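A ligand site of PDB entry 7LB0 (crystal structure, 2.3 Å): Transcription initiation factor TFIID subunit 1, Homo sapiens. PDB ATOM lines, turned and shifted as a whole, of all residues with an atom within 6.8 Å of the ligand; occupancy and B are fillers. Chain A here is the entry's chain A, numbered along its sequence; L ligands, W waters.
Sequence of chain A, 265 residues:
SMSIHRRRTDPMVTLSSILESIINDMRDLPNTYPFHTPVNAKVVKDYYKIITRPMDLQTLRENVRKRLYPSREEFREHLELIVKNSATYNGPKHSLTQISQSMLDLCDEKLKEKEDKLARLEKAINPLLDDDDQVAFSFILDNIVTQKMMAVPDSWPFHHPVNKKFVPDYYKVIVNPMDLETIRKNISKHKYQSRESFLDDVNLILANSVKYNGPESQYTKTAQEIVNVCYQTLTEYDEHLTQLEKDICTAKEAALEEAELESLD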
ATOM      1  N   TRP A 156      19.491 -22.081  21.232  1.00  0.00           N
ATOM      2  CA  TRP A 156      20.213 -20.940  21.784  1.00  0.00           C
ATOM      3  C   TRP A 156      19.489 -20.197  22.915  1.00  0.00           C
ATOM      4  O   TRP A 156      20.181 -19.719  23.824  1.00  0.00           O
ATOM      5  CB  TRP A 156      20.584 -19.958  20.667  1.00  0.00           C
ATOM      6  CG  TRP A 156      19.404 -19.328  20.012  1.00  0.00           C
ATOM      7  CD1 TRP A 156      18.777 -19.765  18.879  1.00  0.00           C
ATOM      8  CD2 TRP A 156      18.686 -18.158  20.438  1.00  0.00           C
ATOM      9  NE1 TRP A 156      17.707 -18.945  18.571  1.00  0.00           N
ATOM     10  CE2 TRP A 156      17.631 -17.955  19.518  1.00  0.00           C
ATOM     11  CE3 TRP A 156      18.816 -17.281  21.517  1.00  0.00           C
ATOM     12  CZ2 TRP A 156      16.718 -16.908  19.646  1.00  0.00           C
ATOM     13  CZ3 TRP A 156      17.910 -16.230  21.639  1.00  0.00           C
ATOM     14  CH2 TRP A 156      16.879 -16.052  20.706  1.00  0.00           C
ATOM     15  N   PRO A 157      18.154 -20.047  22.936  1.00  0.00           N
ATOM     16  CA  PRO A 157      17.547 -19.294  24.060  1.00  0.00           C
ATOM     17  C   PRO A 157      17.828 -19.918  25.418  1.00  0.00           C
ATOM     18  O   PRO A 157      17.711 -19.231  26.443  1.00  0.00           O
ATOM     19  CB  PRO A 157      16.036 -19.319  23.729  1.00  0.00           C
ATOM     20  CG  PRO A 157      15.980 -19.529  22.261  1.00  0.00           C
ATOM     21  CD  PRO A 157      17.100 -20.481  21.993  1.00  0.00           C
ATOM     22  N   PHE A 158      18.181 -21.203  25.437  1.00  0.00           N
ATOM     23  CA  PHE A 158      18.349 -21.946  26.674  1.00  0.00           C
ATOM     24  C   PHE A 158      19.799 -22.222  27.034  1.00  0.00           C
ATOM     25  O   PHE A 158      20.047 -22.890  28.040  1.00  0.00           O
ATOM     26  CB  PHE A 158      17.553 -23.246  26.580  1.00  0.00           C
ATOM     27  CG  PHE A 158      16.128 -23.021  26.190  1.00  0.00           C
ATOM     28  CD1 PHE A 158      15.237 -22.452  27.088  1.00  0.00           C
ATOM     29  CD2 PHE A 158      15.701 -23.312  24.901  1.00  0.00           C
ATOM     30  CE1 PHE A 158      13.917 -22.229  26.734  1.00  0.00           C
ATOM     31  CE2 PHE A 158      14.393 -23.079  24.535  1.00  0.00           C
ATOM     32  CZ  PHE A 158      13.489 -22.537  25.448  1.00  0.00           C
ATOM     33  N   HIS A 159      20.761 -21.728  26.249  1.00  0.00           N
ATOM     34  CA  HIS A 159      22.165 -22.010  26.545  1.00  0.00           C
ATOM     35  C   HIS A 159      22.731 -21.190  27.686  1.00  0.00           C
ATOM     36  O   HIS A 159      23.665 -21.636  28.352  1.00  0.00           O
ATOM     37  CB  HIS A 159      23.027 -21.801  25.301  1.00  0.00           C
ATOM     38  CG  HIS A 159      22.846 -22.846  24.253  1.00  0.00           C
ATOM     39  ND1 HIS A 159      23.827 -23.171  23.341  1.00  0.00           N
ATOM     40  CD2 HIS A 159      21.786 -23.648  23.962  1.00  0.00           C
ATOM     41  CE1 HIS A 159      23.388 -24.133  22.549  1.00  0.00           C
ATOM     42  NE2 HIS A 159      22.150 -24.428  22.899  1.00  0.00           N
ATOM     43  N   HIS A 160      22.175 -20.016  27.972  1.00  0.00           N
ATOM     44  CA  HIS A 160      22.795 -19.116  28.925  1.00  0.00           C
ATOM     45  C   HIS A 160      21.669 -18.467  29.703  1.00  0.00           C
ATOM     46  O   HIS A 160      20.511 -18.483  29.263  1.00  0.00           O
ATOM     47  CB  HIS A 160      23.663 -18.061  28.219  1.00  0.00           C
ATOM     48  CG  HIS A 160      24.730 -18.641  27.357  1.00  0.00           C
ATOM     49  ND1 HIS A 160      25.913 -19.137  27.862  1.00  0.00           N
ATOM     50  CD2 HIS A 160      24.812 -18.786  26.007  1.00  0.00           C
ATOM     51  CE1 HIS A 160      26.673 -19.581  26.867  1.00  0.00           C
ATOM     52  NE2 HIS A 160      26.018 -19.377  25.733  1.00  0.00           N
ATOM     53  N   PRO A 161      21.958 -17.885  30.871  1.00  0.00           N
ATOM     54  CA  PRO A 161      20.926 -17.115  31.579  1.00  0.00           C
ATOM     55  C   PRO A 161      20.444 -15.931  30.752  1.00  0.00           C
ATOM     56  O   PRO A 161      21.239 -15.284  30.063  1.00  0.00           O
ATOM     57  CB  PRO A 161      21.636 -16.654  32.858  1.00  0.00           C
ATOM     58  CG  PRO A 161      22.835 -17.467  32.979  1.00  0.00           C
ATOM     59  CD  PRO A 161      23.231 -17.928  31.618  1.00  0.00           C
ATOM     60  N   VAL A 162      19.139 -15.666  30.826  1.00  0.00           N
ATOM     61  CA  VAL A 162      18.580 -14.483  30.163  1.00  0.00           C
ATOM     62  C   VAL A 162      19.226 -13.235  30.754  1.00  0.00           C
ATOM     63  O   VAL A 162      19.348 -13.091  31.983  1.00  0.00           O
ATOM     64  CB  VAL A 162      17.042 -14.455  30.291  1.00  0.00           C
ATOM     65  CG1 VAL A 162      16.506 -13.121  29.844  1.00  0.00           C
ATOM     66  CG2 VAL A 162      16.420 -15.588  29.492  1.00  0.00           C
ATOM     67  N   ASN A 163      19.603 -12.312  29.883  1.00  0.00           N
ATOM     68  CA  ASN A 163      20.146 -11.016  30.283  1.00  0.00           C
ATOM     69  C   ASN A 163      18.984 -10.041  30.432  1.00  0.00           C
ATOM     70  O   ASN A 163      18.339  -9.662  29.456  1.00  0.00           O
ATOM     71  CB  ASN A 163      21.132 -10.544  29.219  1.00  0.00           C
ATOM     72  CG  ASN A 163      21.969  -9.347  29.655  1.00  0.00           C
ATOM     73  OD1 ASN A 163      21.480  -8.462  30.359  1.00  0.00           O
ATOM     74  ND2 ASN A 163      23.220  -9.322  29.240  1.00  0.00           N
ATOM     75  N   LYS A 164      18.762  -9.586  31.673  1.00  0.00           N
ATOM     76  CA  LYS A 164      17.626  -8.710  31.931  1.00  0.00           C
ATOM     77  C   LYS A 164      17.711  -7.422  31.117  1.00  0.00           C
ATOM     78  O   LYS A 164      16.673  -6.807  30.858  1.00  0.00           O
ATOM     79  CB  LYS A 164      17.551  -8.431  33.436  1.00  0.00           C
ATOM     80  CG  LYS A 164      16.287  -7.686  33.867  1.00  0.00           C
ATOM     81  CD  LYS A 164      15.967  -7.861  35.360  1.00  0.00           C
ATOM     82  CE  LYS A 164      16.960  -7.239  36.292  1.00  0.00           C
ATOM     83  NZ  LYS A 164      16.482  -7.456  37.695  1.00  0.00           N
ATOM     84  N   LYS A 165      18.914  -7.015  30.706  1.00  0.00           N
ATOM     85  CA  LYS A 165      19.039  -5.858  29.831  1.00  0.00           C
ATOM     86  C   LYS A 165      18.304  -6.066  28.512  1.00  0.00           C
ATOM     87  O   LYS A 165      17.746  -5.130  27.933  1.00  0.00           O
ATOM     88  CB  LYS A 165      20.516  -5.547  29.583  1.00  0.00           C
ATOM     89  CG  LYS A 165      20.724  -4.276  28.828  1.00  0.00           C
ATOM     90  CD  LYS A 165      22.186  -3.930  28.623  1.00  0.00           C
ATOM     91  CE  LYS A 165      22.307  -2.499  28.111  1.00  0.00           C
ATOM     92  NZ  LYS A 165      23.689  -2.100  27.774  1.00  0.00           N
ATOM     93  N   PHE A 166      18.299  -7.305  27.996  1.00  0.00           N
ATOM     94  CA  PHE A 166      17.710  -7.589  26.699  1.00  0.00           C
ATOM     95  C   PHE A 166      16.272  -8.094  26.790  1.00  0.00           C
ATOM     96  O   PHE A 166      15.526  -7.949  25.808  1.00  0.00           O
ATOM     97  CB  PHE A 166      18.536  -8.634  25.932  1.00  0.00           C
ATOM     98  CG  PHE A 166      19.966  -8.253  25.706  1.00  0.00           C
ATOM     99  CD1 PHE A 166      20.327  -6.942  25.432  1.00  0.00           C
ATOM    100  CD2 PHE A 166      20.964  -9.225  25.718  1.00  0.00           C
ATOM    101  CE1 PHE A 166      21.666  -6.584  25.229  1.00  0.00           C
ATOM    102  CE2 PHE A 166      22.303  -8.892  25.495  1.00  0.00           C
ATOM    103  CZ  PHE A 166      22.655  -7.567  25.239  1.00  0.00           C
ATOM    104  N   VAL A 167      15.877  -8.679  27.916  1.00  0.00           N
ATOM    105  CA  VAL A 167      14.498  -9.132  28.135  1.00  0.00           C
ATOM    106  C   VAL A 167      14.045  -8.556  29.466  1.00  0.00           C
ATOM    107  O   VAL A 167      14.124  -9.241  30.501  1.00  0.00           O
ATOM    108  CB  VAL A 167      14.357 -10.664  28.107  1.00  0.00           C
ATOM    109  CG1 VAL A 167      12.893 -11.042  28.078  1.00  0.00           C
ATOM    110  CG2 VAL A 167      15.071 -11.287  26.899  1.00  0.00           C
ATOM    111  N   TYR A 170      11.759 -10.496  32.011  1.00  0.00           N
ATOM    112  CA  TYR A 170      11.902 -11.948  32.097  1.00  0.00           C
ATOM    113  C   TYR A 170      11.830 -12.421  33.543  1.00  0.00           C
ATOM    114  O   TYR A 170      11.189 -13.428  33.855  1.00  0.00           O
ATOM    115  CB  TYR A 170      13.212 -12.411  31.465  1.00  0.00           C
ATOM    116  CG  TYR A 170      13.287 -13.916  31.412  1.00  0.00           C
ATOM    117  CD1 TYR A 170      12.563 -14.634  30.480  1.00  0.00           C
ATOM    118  CD2 TYR A 170      14.040 -14.620  32.342  1.00  0.00           C
ATOM    119  CE1 TYR A 170      12.633 -16.011  30.425  1.00  0.00           C
ATOM    120  CE2 TYR A 170      14.110 -16.000  32.316  1.00  0.00           C
ATOM    121  CZ  TYR A 170      13.402 -16.692  31.356  1.00  0.00           C
ATOM    122  OH  TYR A 170      13.470 -18.079  31.323  1.00  0.00           O
ATOM    123  N   TYR A 171      12.496 -11.693  34.443  1.00  0.00           N
ATOM    124  CA  TYR A 171      12.641 -12.145  35.814  1.00  0.00           C
ATOM    125  C   TYR A 171      11.479 -11.698  36.689  1.00  0.00           C
ATOM    126  O   TYR A 171      11.403 -12.092  37.857  1.00  0.00           O
ATOM    127  CB  TYR A 171      14.003 -11.707  36.376  1.00  0.00           C
ATOM    128  CG  TYR A 171      15.156 -12.408  35.664  1.00  0.00           C
ATOM    129  CD1 TYR A 171      15.474 -13.735  35.967  1.00  0.00           C
ATOM    130  CD2 TYR A 171      15.934 -11.762  34.704  1.00  0.00           C
ATOM    131  CE1 TYR A 171      16.500 -14.399  35.319  1.00  0.00           C
ATOM    132  CE2 TYR A 171      16.988 -12.428  34.049  1.00  0.00           C
ATOM    133  CZ  TYR A 171      17.257 -13.746  34.359  1.00  0.00           C
ATOM    134  OH  TYR A 171      18.299 -14.404  33.714  1.00  0.00           O
ATOM    135  N   ASN A 208       9.960 -23.269  32.944  1.00  0.00           N
ATOM    136  CA  ASN A 208      10.077 -21.832  32.733  1.00  0.00           C
ATOM    137  C   ASN A 208       9.716 -21.444  31.310  1.00  0.00           C
ATOM    138  O   ASN A 208       9.166 -20.357  31.090  1.00  0.00           O
ATOM    139  CB  ASN A 208      11.481 -21.364  33.074  1.00  0.00           C
ATOM    140  CG  ASN A 208      11.760 -21.421  34.557  1.00  0.00           C
ATOM    141  OD1 ASN A 208      10.826 -21.417  35.383  1.00  0.00           O
ATOM    142  ND2 ASN A 208      13.031 -21.483  34.921  1.00  0.00           N
ATOM    143  N   SER A 209      10.014 -22.287  30.325  1.00  0.00           N
ATOM    144  CA  SER A 209       9.588 -21.945  28.978  1.00  0.00           C
ATOM    145  C   SER A 209       8.068 -21.999  28.855  1.00  0.00           C
ATOM    146  O   SER A 209       7.459 -21.102  28.259  1.00  0.00           O
ATOM    147  CB  SER A 209      10.241 -22.865  27.947  1.00  0.00           C
ATOM    148  OG  SER A 209       9.901 -22.423  26.648  1.00  0.00           O
ATOM    149  N   TYR A 212       6.849 -18.722  30.647  1.00  0.00           N
ATOM    150  CA  TYR A 212       7.138 -17.420  30.058  1.00  0.00           C
ATOM    151  C   TYR A 212       6.632 -17.311  28.615  1.00  0.00           C
ATOM    152  O   TYR A 212       6.124 -16.251  28.226  1.00  0.00           O
ATOM    153  CB  TYR A 212       8.637 -17.123  30.107  1.00  0.00           C
ATOM    154  CG  TYR A 212       8.938 -15.710  29.677  1.00  0.00           C
ATOM    155  CD1 TYR A 212       8.754 -14.641  30.547  1.00  0.00           C
ATOM    156  CD2 TYR A 212       9.340 -15.435  28.386  1.00  0.00           C
ATOM    157  CE1 TYR A 212       9.002 -13.350  30.147  1.00  0.00           C
ATOM    158  CE2 TYR A 212       9.597 -14.140  27.966  1.00  0.00           C
ATOM    159  CZ  TYR A 212       9.421 -13.106  28.850  1.00  0.00           C
ATOM    160  OH  TYR A 212       9.669 -11.815  28.451  1.00  0.00           O
ATOM    161  N   ASN A 213       6.772 -18.362  27.827  1.00  0.00           N
ATOM    162  CA  ASN A 213       6.460 -18.337  26.397  1.00  0.00           C
ATOM    163  C   ASN A 213       5.121 -18.953  26.071  1.00  0.00           C
ATOM    164  O   ASN A 213       4.569 -18.672  25.000  1.00  0.00           O
ATOM    165  CB  ASN A 213       7.566 -19.061  25.623  1.00  0.00           C
ATOM    166  CG  ASN A 213       8.909 -18.439  25.846  1.00  0.00           C
ATOM    167  OD1 ASN A 213       9.080 -17.241  25.666  1.00  0.00           O
ATOM    168  ND2 ASN A 213       9.871 -19.243  26.299  1.00  0.00           N
ATOM    169  N   SER A 217       4.253 -22.445  22.354  1.00  0.00           N
ATOM    170  CA  SER A 217       5.337 -21.686  21.762  1.00  0.00           C
ATOM    171  C   SER A 217       6.371 -22.593  21.080  1.00  0.00           C
ATOM    172  O   SER A 217       6.591 -23.740  21.488  1.00  0.00           O
ATOM    173  CB  SER A 217       5.965 -20.829  22.849  1.00  0.00           C
ATOM    174  OG  SER A 217       7.210 -20.313  22.450  1.00  0.00           O
ATOM    175  N   TYR A 219       9.470 -21.860  21.269  1.00  0.00           N
ATOM    176  CA  TYR A 219      10.479 -21.942  22.317  1.00  0.00           C
ATOM    177  C   TYR A 219      10.274 -23.171  23.186  1.00  0.00           C
ATOM    178  O   TYR A 219      11.232 -23.890  23.509  1.00  0.00           O
ATOM    179  CB  TYR A 219      10.407 -20.693  23.195  1.00  0.00           C
ATOM    180  CG  TYR A 219      10.879 -19.417  22.557  1.00  0.00           C
ATOM    181  CD1 TYR A 219      10.135 -18.255  22.651  1.00  0.00           C
ATOM    182  CD2 TYR A 219      12.129 -19.350  21.951  1.00  0.00           C
ATOM    183  CE1 TYR A 219      10.571 -17.066  22.103  1.00  0.00           C
ATOM    184  CE2 TYR A 219      12.583 -18.164  21.386  1.00  0.00           C
ATOM    185  CZ  TYR A 219      11.809 -17.023  21.482  1.00  0.00           C
ATOM    186  OH  TYR A 219      12.258 -15.835  20.931  1.00  0.00           O
HETATM  187  C1  LIG L   1      13.288 -16.012  25.215  1.00  0.00           C
HETATM  188  C2  LIG L   1      14.741 -17.189  26.675  1.00  0.00           C
HETATM  189  C3  LIG L   1      16.599 -13.665  24.088  1.00  0.00           C
HETATM  190  C4  LIG L   1      16.738 -10.114  22.629  1.00  0.00           C
HETATM  191  C5  LIG L   1      14.944 -11.281  21.632  1.00  0.00           C
HETATM  192  C6  LIG L   1      14.208 -13.385  21.925  1.00  0.00           C
HETATM  193  C7  LIG L   1      19.461 -15.082  26.055  1.00  0.00           C
HETATM  194  C8  LIG L   1      20.270 -15.994  25.118  1.00  0.00           C
HETATM  195  C9  LIG L   1      20.311 -16.220  26.638  1.00  0.00           C
HETATM  196  C10 LIG L   1      18.072 -14.871  25.402  1.00  0.00           C
HETATM  197  C11 LIG L   1      17.044 -15.779  25.681  1.00  0.00           C
HETATM  198  C12 LIG L   1      15.791 -15.544  25.101  1.00  0.00           C
HETATM  199  C13 LIG L   1      12.911 -14.988  26.325  1.00  0.00           C
HETATM  200  C14 LIG L   1      12.320 -17.187  25.272  1.00  0.00           C
HETATM  201  C15 LIG L   1      13.732 -18.335  26.761  1.00  0.00           C
HETATM  202  C16 LIG L   1      16.293 -12.443  23.224  1.00  0.00           C
HETATM  203  C17 LIG L   1      17.046 -11.249  23.386  1.00  0.00           C
HETATM  204  C18 LIG L   1      15.189 -12.436  22.344  1.00  0.00           C
HETATM  205  C19 LIG L   1      13.410 -12.761  20.985  1.00  0.00           C
HETATM  206  N1  LIG L   1      21.829 -13.544  27.002  1.00  0.00           N
HETATM  207  N2  LIG L   1      14.681 -16.470  25.382  1.00  0.00           N
HETATM  208  N3  LIG L   1      15.599 -14.485  24.334  1.00  0.00           N
HETATM  209  N4  LIG L   1      15.727 -10.154  21.789  1.00  0.00           N
HETATM  210  N5  LIG L   1      13.857 -11.496  20.808  1.00  0.00           N
HETATM  211  N6  LIG L   1      17.823 -13.840  24.623  1.00  0.00           N
HETATM  212  O1  LIG L   1      12.435 -17.903  26.461  1.00  0.00           O
HETATM  213  O2  LIG L   1      19.359 -12.686  27.280  1.00  0.00           O
HETATM  214  O3  LIG L   1      20.183 -12.565  25.187  1.00  0.00           O
HETATM  215  S1  LIG L   1      20.239 -13.441  26.373  1.00  0.00           S
HETATM  216  O   HOH W   1      14.809  -7.395  21.097  1.00  0.00           O
HETATM  217  O   HOH W   2      23.897 -12.470  25.445  1.00  0.00           O
HETATM  218  O   HOH W   3      24.127 -11.692  28.007  1.00  0.00           O
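Water W3 lies within hydrogen-bond range of the side-chain amide nitrogen of Asn 163 (2.8 Å) and a nitrogen (N1) of the ligand (3.1 Å).
ND2 of Asn 213 lies within hydrogen-bond range of O1 of the ligand, 2.9 Å away. N of Asn 163 is in hydrogen-bond range of O2 of the ligand (2.6 Å).
CZ3 of Trp 156 touches C3 of the ligand, 3.8 Å away. CB of Pro 157 touches N2 of the ligand (3.6 Å). Phe 158 touches the ligand. O of His 160 touches C9 of the ligand, at 3.5 Å. O of Pro 161 touches N1 of the ligand (3.6 Å). Val 162 touches the ligand. Phe 166 touches the ligand (CD2 to O3, 3.5 Å). Val 167 touches the ligand (CG2 to C3, 3.99 Å). Tyr 212 touches the ligand (CE2 to C13, 3.8 Å). OH of Tyr 219 touches C19 of the ligand (3.3 Å). Hydrophobic or aromatic side chains that line the ligand: Trp 156, Pro 157, Phe 158, Val 162, Phe 166, Val 167, Tyr 212 and Tyr 219. Of the 20 residues printed, 12 come within 4 Å of the ligand.
The backbone carbonyl oxygen (O) of Val 162 lies within hydrogen-bond range of the side-chain hydroxyl (OH) of Tyr 171, at 2.4 Å. ND2 of Asn 213 is in hydrogen-bond range of OG of Ser 209, at 3.2 Å. The backbone NH of Tyr 219 lies within hydrogen-bond range of the side-chain hydroxyl of Ser 217 (3.0 Å). The side-chain amide oxygen (OD1) of Asn 163 lies within hydrogen-bond range of the backbone NH (N) of Lys 165, 3.0 Å away.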
